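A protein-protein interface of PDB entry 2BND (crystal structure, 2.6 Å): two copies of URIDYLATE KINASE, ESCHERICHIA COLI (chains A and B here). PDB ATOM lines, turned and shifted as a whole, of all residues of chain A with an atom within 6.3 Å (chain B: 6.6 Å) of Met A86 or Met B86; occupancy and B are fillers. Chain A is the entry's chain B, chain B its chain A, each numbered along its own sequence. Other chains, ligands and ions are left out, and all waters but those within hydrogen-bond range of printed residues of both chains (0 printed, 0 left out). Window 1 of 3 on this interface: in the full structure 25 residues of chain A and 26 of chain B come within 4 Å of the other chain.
Ile A29 touches Met B79, and with the chains exchanged Met A79 touches Ile B29.
Phe A61 touches Met B86, and with the chains exchanged Met A86 touches Phe B61.
Met A79 touches Leu B89, and with the chains exchanged Leu A89 touches Met B79.
Leu A82 touches its own counterpart, Leu B82.
Of the 22 pairs that touch across the chains among the printed residues, 18 have their exchanged pair printed and touching as well.
Printed residues of chain A that touch a printed residue of chain B: Ile A29, Leu A60, Phe A61, Met A79, Leu A82, Val A85, Met A86, Leu A89 and Ala A90.
Along chain A the printed residues that touch a printed residue of chain B span positions 29 to 90.
Printed residues of chain B that touch a printed residue of chain A: Ile B29, Leu B60, Phe B61, Met B71, Met B79, Leu B82, Ala B83, Val B85, Met B86 and Leu B89.
Hydrophobic or aromatic side chains of chain B within 4 Å of the printed part of chain A: Ile B29, Leu B60, Phe B61, Met B71, Met B79, Leu B82, Ala B83, Val B85, Met B86 and Leu B89.
Among the printed residues, no Asp or Glu carboxylate lies within 4 Å of a Lys or Arg side-chain nitrogen of the other chain.
Printed residues of chain B within 4 Å of Met A86: Phe B61, Met B79, Leu B82, Ala B83 and Met B86.
Of chain A, only Phe A61, Met A79, Leu A82 and Met A86 come within 4 Å of Met B86.
Of the printed residues of chain B, Ala A90 touches Met B71 and Met B79.
Of the printed residues of chain A, Leu B60 touches Phe A61.
Thr B84 touches none of the printed residues of chain A.
Ser B135 touches none of the printed residues of chain A.
The nearest residue of chain A that does not touch Met B86 is Ala A83 (4.1 Å).
The side-chain sulfur of Met A86 lies close to the side-chain sulfur of Met B86 (3.2 Å).
CD1 of Ile A29 touches CZ of Phe B61, 3.9 Å away.
Ile A29 touches Met B79.
Leu A60 touches Phe B61 (CD2 to CZ, 3.5 Å).
Met B86 touches Phe A61.
Met A79 touches Ile B29 (CE to CD1, 3.5 Å).
CG1 of Val A85 touches CD1 of Leu B82 (3.7 Å).
CD1 of Phe B61 touches CE of Met A86, at 3.4 Å.
Met A86 touches Met B79 (O to CE, 2.9 Å).
Leu B82 touches Met A86.
Met B79 touches Ala A90 (CE to CB, 3.5 Å).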
ATOM      1  N   ILE A  29       2.833  -0.376 -20.294  1.00  0.00           N
ATOM      2  CA  ILE A  29       1.878  -1.276 -19.658  1.00  0.00           C
ATOM      3  C   ILE A  29       1.860  -2.604 -20.382  1.00  0.00           C
ATOM      4  O   ILE A  29       1.920  -2.644 -21.602  1.00  0.00           O
ATOM      5  CB  ILE A  29       0.452  -0.687 -19.700  1.00  0.00           C
ATOM      6  CG1 ILE A  29       0.462   0.728 -19.130  1.00  0.00           C
ATOM      7  CG2 ILE A  29      -0.500  -1.568 -18.918  1.00  0.00           C
ATOM      8  CD1 ILE A  29      -0.873   1.433 -19.241  1.00  0.00           C
ATOM      9  N   LEU A  60       5.500   4.464 -15.396  1.00  0.00           N
ATOM     10  CA  LEU A  60       5.541   5.635 -16.267  1.00  0.00           C
ATOM     11  C   LEU A  60       6.388   6.779 -15.685  1.00  0.00           C
ATOM     12  O   LEU A  60       7.369   7.200 -16.294  1.00  0.00           O
ATOM     13  CB  LEU A  60       4.114   6.111 -16.548  1.00  0.00           C
ATOM     14  CG  LEU A  60       3.174   5.010 -17.080  1.00  0.00           C
ATOM     15  CD1 LEU A  60       1.726   5.477 -17.033  1.00  0.00           C
ATOM     16  CD2 LEU A  60       3.572   4.627 -18.499  1.00  0.00           C
ATOM     17  N   PHE A  61       6.024   7.279 -14.509  1.00  0.00           N
ATOM     18  CA  PHE A  61       6.786   8.364 -13.904  1.00  0.00           C
ATOM     19  C   PHE A  61       6.741   8.405 -12.389  1.00  0.00           C
ATOM     20  O   PHE A  61       5.764   8.009 -11.760  1.00  0.00           O
ATOM     21  CB  PHE A  61       6.292   9.738 -14.375  1.00  0.00           C
ATOM     22  CG  PHE A  61       6.414   9.969 -15.841  1.00  0.00           C
ATOM     23  CD1 PHE A  61       5.317   9.804 -16.671  1.00  0.00           C
ATOM     24  CD2 PHE A  61       7.620  10.395 -16.390  1.00  0.00           C
ATOM     25  CE1 PHE A  61       5.413  10.064 -18.029  1.00  0.00           C
ATOM     26  CE2 PHE A  61       7.728  10.658 -17.734  1.00  0.00           C
ATOM     27  CZ  PHE A  61       6.622  10.494 -18.562  1.00  0.00           C
ATOM     28  N   HIS A  78       2.766  15.588  -9.942  1.00  0.00           N
ATOM     29  CA  HIS A  78       1.543  15.734 -10.720  1.00  0.00           C
ATOM     30  C   HIS A  78       1.594  14.753 -11.892  1.00  0.00           C
ATOM     31  O   HIS A  78       0.672  13.969 -12.110  1.00  0.00           O
ATOM     32  CB  HIS A  78       1.394  17.173 -11.235  1.00  0.00           C
ATOM     33  CG  HIS A  78       0.932  18.153 -10.195  1.00  0.00           C
ATOM     34  ND1 HIS A  78       0.596  19.456 -10.498  1.00  0.00           N
ATOM     35  CD2 HIS A  78       0.765  18.027  -8.856  1.00  0.00           C
ATOM     36  CE1 HIS A  78       0.247  20.088  -9.391  1.00  0.00           C
ATOM     37  NE2 HIS A  78       0.341  19.244  -8.381  1.00  0.00           N
ATOM     38  N   MET A  79       2.677  14.796 -12.654  1.00  0.00           N
ATOM     39  CA  MET A  79       2.814  13.871 -13.760  1.00  0.00           C
ATOM     40  C   MET A  79       2.684  12.457 -13.203  1.00  0.00           C
ATOM     41  O   MET A  79       1.971  11.618 -13.758  1.00  0.00           O
ATOM     42  CB  MET A  79       4.168  14.055 -14.431  1.00  0.00           C
ATOM     43  CG  MET A  79       4.200  15.214 -15.404  1.00  0.00           C
ATOM     44  SD  MET A  79       5.878  15.667 -15.846  1.00  0.00           S
ATOM     45  CE  MET A  79       6.274  14.377 -17.037  1.00  0.00           C
ATOM     46  N   GLY A  80       3.371  12.203 -12.093  1.00  0.00           N
ATOM     47  CA  GLY A  80       3.309  10.891 -11.489  1.00  0.00           C
ATOM     48  C   GLY A  80       1.873  10.486 -11.216  1.00  0.00           C
ATOM     49  O   GLY A  80       1.418   9.410 -11.636  1.00  0.00           O
ATOM     50  N   MET A  81       1.151  11.360 -10.517  1.00  0.00           N
ATOM     51  CA  MET A  81      -0.238  11.086 -10.186  1.00  0.00           C
ATOM     52  C   MET A  81      -1.074  10.877 -11.426  1.00  0.00           C
ATOM     53  O   MET A  81      -2.023  10.105 -11.401  1.00  0.00           O
ATOM     54  CB  MET A  81      -0.835  12.218  -9.347  1.00  0.00           C
ATOM     55  CG  MET A  81      -0.356  12.223  -7.905  1.00  0.00           C
ATOM     56  SD  MET A  81      -1.206  13.402  -6.853  1.00  0.00           S
ATOM     57  CE  MET A  81      -0.226  14.842  -7.094  1.00  0.00           C
ATOM     58  N   LEU A  82      -0.716  11.549 -12.515  1.00  0.00           N
ATOM     59  CA  LEU A  82      -1.475  11.414 -13.755  1.00  0.00           C
ATOM     60  C   LEU A  82      -1.211  10.060 -14.391  1.00  0.00           C
ATOM     61  O   LEU A  82      -2.030   9.555 -15.152  1.00  0.00           O
ATOM     62  CB  LEU A  82      -1.114  12.534 -14.729  1.00  0.00           C
ATOM     63  CG  LEU A  82      -2.278  13.153 -15.512  1.00  0.00           C
ATOM     64  CD1 LEU A  82      -1.760  14.338 -16.321  1.00  0.00           C
ATOM     65  CD2 LEU A  82      -2.924  12.120 -16.435  1.00  0.00           C
ATOM     66  N   ALA A  83      -0.061   9.470 -14.076  1.00  0.00           N
ATOM     67  CA  ALA A  83       0.283   8.156 -14.610  1.00  0.00           C
ATOM     68  C   ALA A  83      -0.632   7.116 -13.957  1.00  0.00           C
ATOM     69  O   ALA A  83      -1.124   6.203 -14.618  1.00  0.00           O
ATOM     70  CB  ALA A  83       1.738   7.836 -14.326  1.00  0.00           C
ATOM     71  N   THR A  84      -0.859   7.265 -12.657  1.00  0.00           N
ATOM     72  CA  THR A  84      -1.729   6.344 -11.938  1.00  0.00           C
ATOM     73  C   THR A  84      -3.101   6.320 -12.617  1.00  0.00           C
ATOM     74  O   THR A  84      -3.697   5.256 -12.780  1.00  0.00           O
ATOM     75  CB  THR A  84      -1.916   6.763 -10.467  1.00  0.00           C
ATOM     76  OG1 THR A  84      -2.631   8.001 -10.410  1.00  0.00           O
ATOM     77  CG2 THR A  84      -0.559   6.929  -9.782  1.00  0.00           C
ATOM     78  N   VAL A  85      -3.593   7.488 -13.014  1.00  0.00           N
ATOM     79  CA  VAL A  85      -4.878   7.574 -13.684  1.00  0.00           C
ATOM     80  C   VAL A  85      -4.798   6.818 -15.010  1.00  0.00           C
ATOM     81  O   VAL A  85      -5.687   6.033 -15.352  1.00  0.00           O
ATOM     82  CB  VAL A  85      -5.262   9.043 -13.950  1.00  0.00           C
ATOM     83  CG1 VAL A  85      -6.573   9.117 -14.713  1.00  0.00           C
ATOM     84  CG2 VAL A  85      -5.364   9.793 -12.629  1.00  0.00           C
ATOM     85  N   MET A  86      -3.722   7.056 -15.753  1.00  0.00           N
ATOM     86  CA  MET A  86      -3.526   6.368 -17.018  1.00  0.00           C
ATOM     87  C   MET A  86      -3.565   4.862 -16.755  1.00  0.00           C
ATOM     88  O   MET A  86      -4.163   4.109 -17.527  1.00  0.00           O
ATOM     89  CB  MET A  86      -2.185   6.773 -17.644  1.00  0.00           C
ATOM     90  CG  MET A  86      -2.128   8.247 -18.038  1.00  0.00           C
ATOM     91  SD  MET A  86      -0.561   8.779 -18.795  1.00  0.00           S
ATOM     92  CE  MET A  86      -0.919   8.439 -20.521  1.00  0.00           C
ATOM     93  N   ASN A  87      -2.934   4.422 -15.663  1.00  0.00           N
ATOM     94  CA  ASN A  87      -2.936   2.996 -15.323  1.00  0.00           C
ATOM     95  C   ASN A  87      -4.326   2.566 -14.864  1.00  0.00           C
ATOM     96  O   ASN A  87      -4.755   1.439 -15.110  1.00  0.00           O
ATOM     97  CB  ASN A  87      -1.925   2.676 -14.210  1.00  0.00           C
ATOM     98  CG  ASN A  87      -0.494   2.565 -14.718  1.00  0.00           C
ATOM     99  OD1 ASN A  87      -0.256   2.145 -15.851  1.00  0.00           O
ATOM    100  ND2 ASN A  87       0.469   2.921 -13.866  1.00  0.00           N
ATOM    101  N   GLY A  88      -5.024   3.475 -14.190  1.00  0.00           N
ATOM    102  CA  GLY A  88      -6.355   3.168 -13.709  1.00  0.00           C
ATOM    103  C   GLY A  88      -7.298   3.012 -14.876  1.00  0.00           C
ATOM    104  O   GLY A  88      -8.283   2.278 -14.806  1.00  0.00           O
ATOM    105  N   LEU A  89      -6.988   3.706 -15.961  1.00  0.00           N
ATOM    106  CA  LEU A  89      -7.811   3.655 -17.162  1.00  0.00           C
ATOM    107  C   LEU A  89      -7.667   2.279 -17.812  1.00  0.00           C
ATOM    108  O   LEU A  89      -8.656   1.629 -18.136  1.00  0.00           O
ATOM    109  CB  LEU A  89      -7.368   4.758 -18.126  1.00  0.00           C
ATOM    110  CG  LEU A  89      -8.387   5.679 -18.794  1.00  0.00           C
ATOM    111  CD1 LEU A  89      -9.723   5.630 -18.087  1.00  0.00           C
ATOM    112  CD2 LEU A  89      -7.828   7.101 -18.777  1.00  0.00           C
ATOM    113  N   ALA A  90      -6.428   1.826 -17.985  1.00  0.00           N
ATOM    114  CA  ALA A  90      -6.180   0.526 -18.595  1.00  0.00           C
ATOM    115  C   ALA A  90      -6.695  -0.615 -17.714  1.00  0.00           C
ATOM    116  O   ALA A  90      -7.243  -1.592 -18.221  1.00  0.00           O
ATOM    117  CB  ALA A  90      -4.686   0.348 -18.880  1.00  0.00           C
ATOM    118  N   MET A  91      -6.525  -0.506 -16.401  1.00  0.00           N
ATOM    119  CA  MET A  91      -7.020  -1.566 -15.528  1.00  0.00           C
ATOM    120  C   MET A  91      -8.549  -1.638 -15.587  1.00  0.00           C
ATOM    121  O   MET A  91      -9.121  -2.727 -15.598  1.00  0.00           O
ATOM    122  CB  MET A  91      -6.568  -1.358 -14.083  1.00  0.00           C
ATOM    123  CG  MET A  91      -7.034  -2.460 -13.114  1.00  0.00           C
ATOM    124  SD  MET A  91      -6.385  -4.148 -13.427  1.00  0.00           S
ATOM    125  CE  MET A  91      -4.722  -3.808 -13.783  1.00  0.00           C
ATOM    126  N   LEU A 104     -13.776   4.019 -12.131  1.00  0.00           N
ATOM    127  CA  LEU A 104     -12.492   4.635 -11.825  1.00  0.00           C
ATOM    128  C   LEU A 104     -12.702   6.020 -11.250  1.00  0.00           C
ATOM    129  O   LEU A 104     -13.397   6.844 -11.847  1.00  0.00           O
ATOM    130  CB  LEU A 104     -11.635   4.752 -13.089  1.00  0.00           C
ATOM    131  CG  LEU A 104     -10.324   5.535 -12.955  1.00  0.00           C
ATOM    132  CD1 LEU A 104      -9.386   4.812 -11.993  1.00  0.00           C
ATOM    133  CD2 LEU A 104      -9.671   5.672 -14.328  1.00  0.00           C
ATOM    134  N   SER A 135      -7.261   6.270  -8.408  1.00  0.00           N
ATOM    135  CA  SER A 135      -6.036   6.737  -9.039  1.00  0.00           C
ATOM    136  C   SER A 135      -5.670   8.117  -8.474  1.00  0.00           C
ATOM    137  O   SER A 135      -6.446   8.712  -7.726  1.00  0.00           O
ATOM    138  CB  SER A 135      -6.228   6.801 -10.556  1.00  0.00           C
ATOM    139  OG  SER A 135      -7.239   7.736 -10.901  1.00  0.00           O
ATOM    140  N   ILE B  29      10.387  11.114 -21.360  1.00  0.00           N
ATOM    141  CA  ILE B  29      10.791  12.482 -21.635  1.00  0.00           C
ATOM    142  C   ILE B  29      12.263  12.677 -21.311  1.00  0.00           C
ATOM    143  O   ILE B  29      12.783  12.088 -20.366  1.00  0.00           O
ATOM    144  CB  ILE B  29       9.985  13.473 -20.778  1.00  0.00           C
ATOM    145  CG1 ILE B  29       8.490  13.293 -21.029  1.00  0.00           C
ATOM    146  CG2 ILE B  29      10.380  14.883 -21.117  1.00  0.00           C
ATOM    147  CD1 ILE B  29       7.619  14.259 -20.246  1.00  0.00           C
ATOM    148  N   LEU B  60       4.713   8.279 -25.292  1.00  0.00           N
ATOM    149  CA  LEU B  60       4.083   7.537 -24.208  1.00  0.00           C
ATOM    150  C   LEU B  60       3.049   6.529 -24.710  1.00  0.00           C
ATOM    151  O   LEU B  60       3.227   5.321 -24.545  1.00  0.00           O
ATOM    152  CB  LEU B  60       3.427   8.496 -23.212  1.00  0.00           C
ATOM    153  CG  LEU B  60       4.375   9.334 -22.353  1.00  0.00           C
ATOM    154  CD1 LEU B  60       3.619  10.472 -21.693  1.00  0.00           C
ATOM    155  CD2 LEU B  60       5.023   8.450 -21.302  1.00  0.00           C
ATOM    156  N   PHE B  61       1.977   7.019 -25.325  1.00  0.00           N
ATOM    157  CA  PHE B  61       0.923   6.143 -25.807  1.00  0.00           C
ATOM    158  C   PHE B  61       0.187   6.645 -27.042  1.00  0.00           C
ATOM    159  O   PHE B  61       0.084   7.846 -27.287  1.00  0.00           O
ATOM    160  CB  PHE B  61      -0.144   5.921 -24.723  1.00  0.00           C
ATOM    161  CG  PHE B  61       0.363   5.271 -23.472  1.00  0.00           C
ATOM    162  CD1 PHE B  61       0.666   6.040 -22.347  1.00  0.00           C
ATOM    163  CD2 PHE B  61       0.511   3.885 -23.402  1.00  0.00           C
ATOM    164  CE1 PHE B  61       1.104   5.440 -21.170  1.00  0.00           C
ATOM    165  CE2 PHE B  61       0.943   3.283 -22.239  1.00  0.00           C
ATOM    166  CZ  PHE B  61       1.241   4.063 -21.116  1.00  0.00           C
ATOM    167  N   MET B  71      -7.193  -3.562 -25.908  1.00  0.00           N
ATOM    168  CA  MET B  71      -7.930  -2.534 -25.173  1.00  0.00           C
ATOM    169  C   MET B  71      -8.939  -1.786 -26.055  1.00  0.00           C
ATOM    170  O   MET B  71      -8.754  -1.685 -27.270  1.00  0.00           O
ATOM    171  CB  MET B  71      -6.933  -1.540 -24.574  1.00  0.00           C
ATOM    172  CG  MET B  71      -7.541  -0.360 -23.835  1.00  0.00           C
ATOM    173  SD  MET B  71      -6.258   0.809 -23.317  1.00  0.00           S
ATOM    174  CE  MET B  71      -5.414  -0.177 -22.109  1.00  0.00           C
ATOM    175  N   HIS B  78      -8.141   7.811 -24.954  1.00  0.00           N
ATOM    176  CA  HIS B  78      -8.248   8.639 -23.767  1.00  0.00           C
ATOM    177  C   HIS B  78      -6.865   8.689 -23.115  1.00  0.00           C
ATOM    178  O   HIS B  78      -6.301   9.758 -22.918  1.00  0.00           O
ATOM    179  CB  HIS B  78      -9.302   8.068 -22.802  1.00  0.00           C
ATOM    180  CG  HIS B  78     -10.710   8.470 -23.132  1.00  0.00           C
ATOM    181  ND1 HIS B  78     -11.806   7.964 -22.465  1.00  0.00           N
ATOM    182  CD2 HIS B  78     -11.201   9.317 -24.069  1.00  0.00           C
ATOM    183  CE1 HIS B  78     -12.909   8.479 -22.979  1.00  0.00           C
ATOM    184  NE2 HIS B  78     -12.570   9.302 -23.955  1.00  0.00           N
ATOM    185  N   MET B  79      -6.318   7.524 -22.798  1.00  0.00           N
ATOM    186  CA  MET B  79      -5.000   7.438 -22.196  1.00  0.00           C
ATOM    187  C   MET B  79      -3.984   8.204 -23.052  1.00  0.00           C
ATOM    188  O   MET B  79      -3.094   8.885 -22.533  1.00  0.00           O
ATOM    189  CB  MET B  79      -4.573   5.978 -22.098  1.00  0.00           C
ATOM    190  CG  MET B  79      -5.345   5.152 -21.095  1.00  0.00           C
ATOM    191  SD  MET B  79      -4.859   3.424 -21.226  1.00  0.00           S
ATOM    192  CE  MET B  79      -3.430   3.374 -20.226  1.00  0.00           C
ATOM    193  N   GLY B  80      -4.116   8.077 -24.366  1.00  0.00           N
ATOM    194  CA  GLY B  80      -3.210   8.773 -25.256  1.00  0.00           C
ATOM    195  C   GLY B  80      -3.352  10.270 -25.076  1.00  0.00           C
ATOM    196  O   GLY B  80      -2.369  11.009 -25.129  1.00  0.00           O
ATOM    197  N   MET B  81      -4.581  10.728 -24.870  1.00  0.00           N
ATOM    198  CA  MET B  81      -4.800  12.146 -24.676  1.00  0.00           C
ATOM    199  C   MET B  81      -4.158  12.558 -23.359  1.00  0.00           C
ATOM    200  O   MET B  81      -3.418  13.547 -23.301  1.00  0.00           O
ATOM    201  CB  MET B  81      -6.299  12.475 -24.688  1.00  0.00           C
ATOM    202  CG  MET B  81      -6.930  12.328 -26.076  1.00  0.00           C
ATOM    203  SD  MET B  81      -8.412  13.320 -26.374  1.00  0.00           S
ATOM    204  CE  MET B  81      -9.700  12.142 -26.131  1.00  0.00           C
ATOM    205  N   LEU B  82      -4.414  11.785 -22.306  1.00  0.00           N
ATOM    206  CA  LEU B  82      -3.842  12.104 -21.009  1.00  0.00           C
ATOM    207  C   LEU B  82      -2.348  12.235 -21.163  1.00  0.00           C
ATOM    208  O   LEU B  82      -1.716  13.020 -20.465  1.00  0.00           O
ATOM    209  CB  LEU B  82      -4.153  11.020 -19.973  1.00  0.00           C
ATOM    210  CG  LEU B  82      -5.562  10.978 -19.376  1.00  0.00           C
ATOM    211  CD1 LEU B  82      -5.582   9.982 -18.216  1.00  0.00           C
ATOM    212  CD2 LEU B  82      -5.978  12.361 -18.882  1.00  0.00           C
ATOM    213  N   ALA B  83      -1.785  11.466 -22.089  1.00  0.00           N
ATOM    214  CA  ALA B  83      -0.352  11.507 -22.327  1.00  0.00           C
ATOM    215  C   ALA B  83       0.045  12.895 -22.838  1.00  0.00           C
ATOM    216  O   ALA B  83       1.015  13.487 -22.353  1.00  0.00           O
ATOM    217  CB  ALA B  83       0.041  10.436 -23.323  1.00  0.00           C
ATOM    218  N   THR B  84      -0.702  13.420 -23.808  1.00  0.00           N
ATOM    219  CA  THR B  84      -0.399  14.750 -24.334  1.00  0.00           C
ATOM    220  C   THR B  84      -0.344  15.710 -23.148  1.00  0.00           C
ATOM    221  O   THR B  84       0.552  16.549 -23.058  1.00  0.00           O
ATOM    222  CB  THR B  84      -1.476  15.253 -25.325  1.00  0.00           C
ATOM    223  OG1 THR B  84      -2.729  15.385 -24.643  1.00  0.00           O
ATOM    224  CG2 THR B  84      -1.635  14.290 -26.484  1.00  0.00           C
ATOM    225  N   VAL B  85      -1.300  15.572 -22.234  1.00  0.00           N
ATOM    226  CA  VAL B  85      -1.338  16.410 -21.038  1.00  0.00           C
ATOM    227  C   VAL B  85      -0.070  16.178 -20.210  1.00  0.00           C
ATOM    228  O   VAL B  85       0.548  17.137 -19.737  1.00  0.00           O
ATOM    229  CB  VAL B  85      -2.587  16.099 -20.164  1.00  0.00           C
ATOM    230  CG1 VAL B  85      -2.584  16.973 -18.904  1.00  0.00           C
ATOM    231  CG2 VAL B  85      -3.849  16.341 -20.966  1.00  0.00           C
ATOM    232  N   MET B  86       0.323  14.916 -20.040  1.00  0.00           N
ATOM    233  CA  MET B  86       1.536  14.614 -19.283  1.00  0.00           C
ATOM    234  C   MET B  86       2.748  15.304 -19.896  1.00  0.00           C
ATOM    235  O   MET B  86       3.654  15.711 -19.174  1.00  0.00           O
ATOM    236  CB  MET B  86       1.788  13.108 -19.212  1.00  0.00           C
ATOM    237  CG  MET B  86       0.805  12.380 -18.309  1.00  0.00           C
ATOM    238  SD  MET B  86       1.484  10.883 -17.578  1.00  0.00           S
ATOM    239  CE  MET B  86       2.736  11.641 -16.525  1.00  0.00           C
ATOM    240  N   ASN B  87       2.768  15.429 -21.225  1.00  0.00           N
ATOM    241  CA  ASN B  87       3.869  16.102 -21.901  1.00  0.00           C
ATOM    242  C   ASN B  87       3.775  17.602 -21.637  1.00  0.00           C
ATOM    243  O   ASN B  87       4.764  18.241 -21.255  1.00  0.00           O
ATOM    244  CB  ASN B  87       3.838  15.846 -23.413  1.00  0.00           C
ATOM    245  CG  ASN B  87       4.390  14.479 -23.790  1.00  0.00           C
ATOM    246  OD1 ASN B  87       5.364  14.004 -23.200  1.00  0.00           O
ATOM    247  ND2 ASN B  87       3.777  13.848 -24.790  1.00  0.00           N
ATOM    248  N   GLY B  88       2.581  18.154 -21.835  1.00  0.00           N
ATOM    249  CA  GLY B  88       2.371  19.574 -21.608  1.00  0.00           C
ATOM    250  C   GLY B  88       2.906  19.985 -20.251  1.00  0.00           C
ATOM    251  O   GLY B  88       3.542  21.030 -20.113  1.00  0.00           O
ATOM    252  N   LEU B  89       2.643  19.157 -19.243  1.00  0.00           N
ATOM    253  CA  LEU B  89       3.121  19.429 -17.895  1.00  0.00           C
ATOM    254  C   LEU B  89       4.625  19.632 -17.950  1.00  0.00           C
ATOM    255  O   LEU B  89       5.159  20.597 -17.401  1.00  0.00           O
ATOM    256  CB  LEU B  89       2.810  18.247 -16.983  1.00  0.00           C
ATOM    257  CG  LEU B  89       1.692  18.363 -15.950  1.00  0.00           C
ATOM    258  CD1 LEU B  89       0.838  19.555 -16.241  1.00  0.00           C
ATOM    259  CD2 LEU B  89       0.865  17.086 -15.959  1.00  0.00           C
ATOM    260  N   ALA B  90       5.304  18.706 -18.623  1.00  0.00           N
ATOM    261  CA  ALA B  90       6.753  18.771 -18.749  1.00  0.00           C
ATOM    262  C   ALA B  90       7.177  20.012 -19.524  1.00  0.00           C
ATOM    263  O   ALA B  90       8.058  20.741 -19.098  1.00  0.00           O
ATOM    264  CB  ALA B  90       7.272  17.519 -19.423  1.00  0.00           C
ATOM    265  N   MET B  91       6.542  20.259 -20.660  1.00  0.00           N
ATOM    266  CA  MET B  91       6.899  21.433 -21.440  1.00  0.00           C
ATOM    267  C   MET B  91       6.714  22.718 -20.616  1.00  0.00           C
ATOM    268  O   MET B  91       7.610  23.563 -20.565  1.00  0.00           O
ATOM    269  CB  MET B  91       6.067  21.490 -22.716  1.00  0.00           C
ATOM    270  CG  MET B  91       6.475  22.602 -23.676  1.00  0.00           C
ATOM    271  SD  MET B  91       8.259  22.738 -23.923  1.00  0.00           S
ATOM    272  CE  MET B  91       8.537  21.493 -25.144  1.00  0.00           C
ATOM    273  N   LEU B 104      -0.691  25.930 -19.181  1.00  0.00           N
ATOM    274  CA  LEU B 104      -1.198  24.712 -19.785  1.00  0.00           C
ATOM    275  C   LEU B 104      -2.718  24.687 -19.705  1.00  0.00           C
ATOM    276  O   LEU B 104      -3.303  24.971 -18.662  1.00  0.00           O
ATOM    277  CB  LEU B 104      -0.628  23.494 -19.061  1.00  0.00           C
ATOM    278  CG  LEU B 104      -1.189  22.111 -19.413  1.00  0.00           C
ATOM    279  CD1 LEU B 104      -0.885  21.717 -20.860  1.00  0.00           C
ATOM    280  CD2 LEU B 104      -0.557  21.119 -18.476  1.00  0.00           C
ATOM    281  N   SER B 135      -2.972  20.920 -24.501  1.00  0.00           N
ATOM    282  CA  SER B 135      -2.865  19.466 -24.433  1.00  0.00           C
ATOM    283  C   SER B 135      -4.220  18.737 -24.597  1.00  0.00           C
ATOM    284  O   SER B 135      -5.251  19.360 -24.863  1.00  0.00           O
ATOM    285  CB  SER B 135      -2.200  19.066 -23.114  1.00  0.00           C
ATOM    286  OG  SER B 135      -2.829  19.707 -22.019  1.00  0.00           O
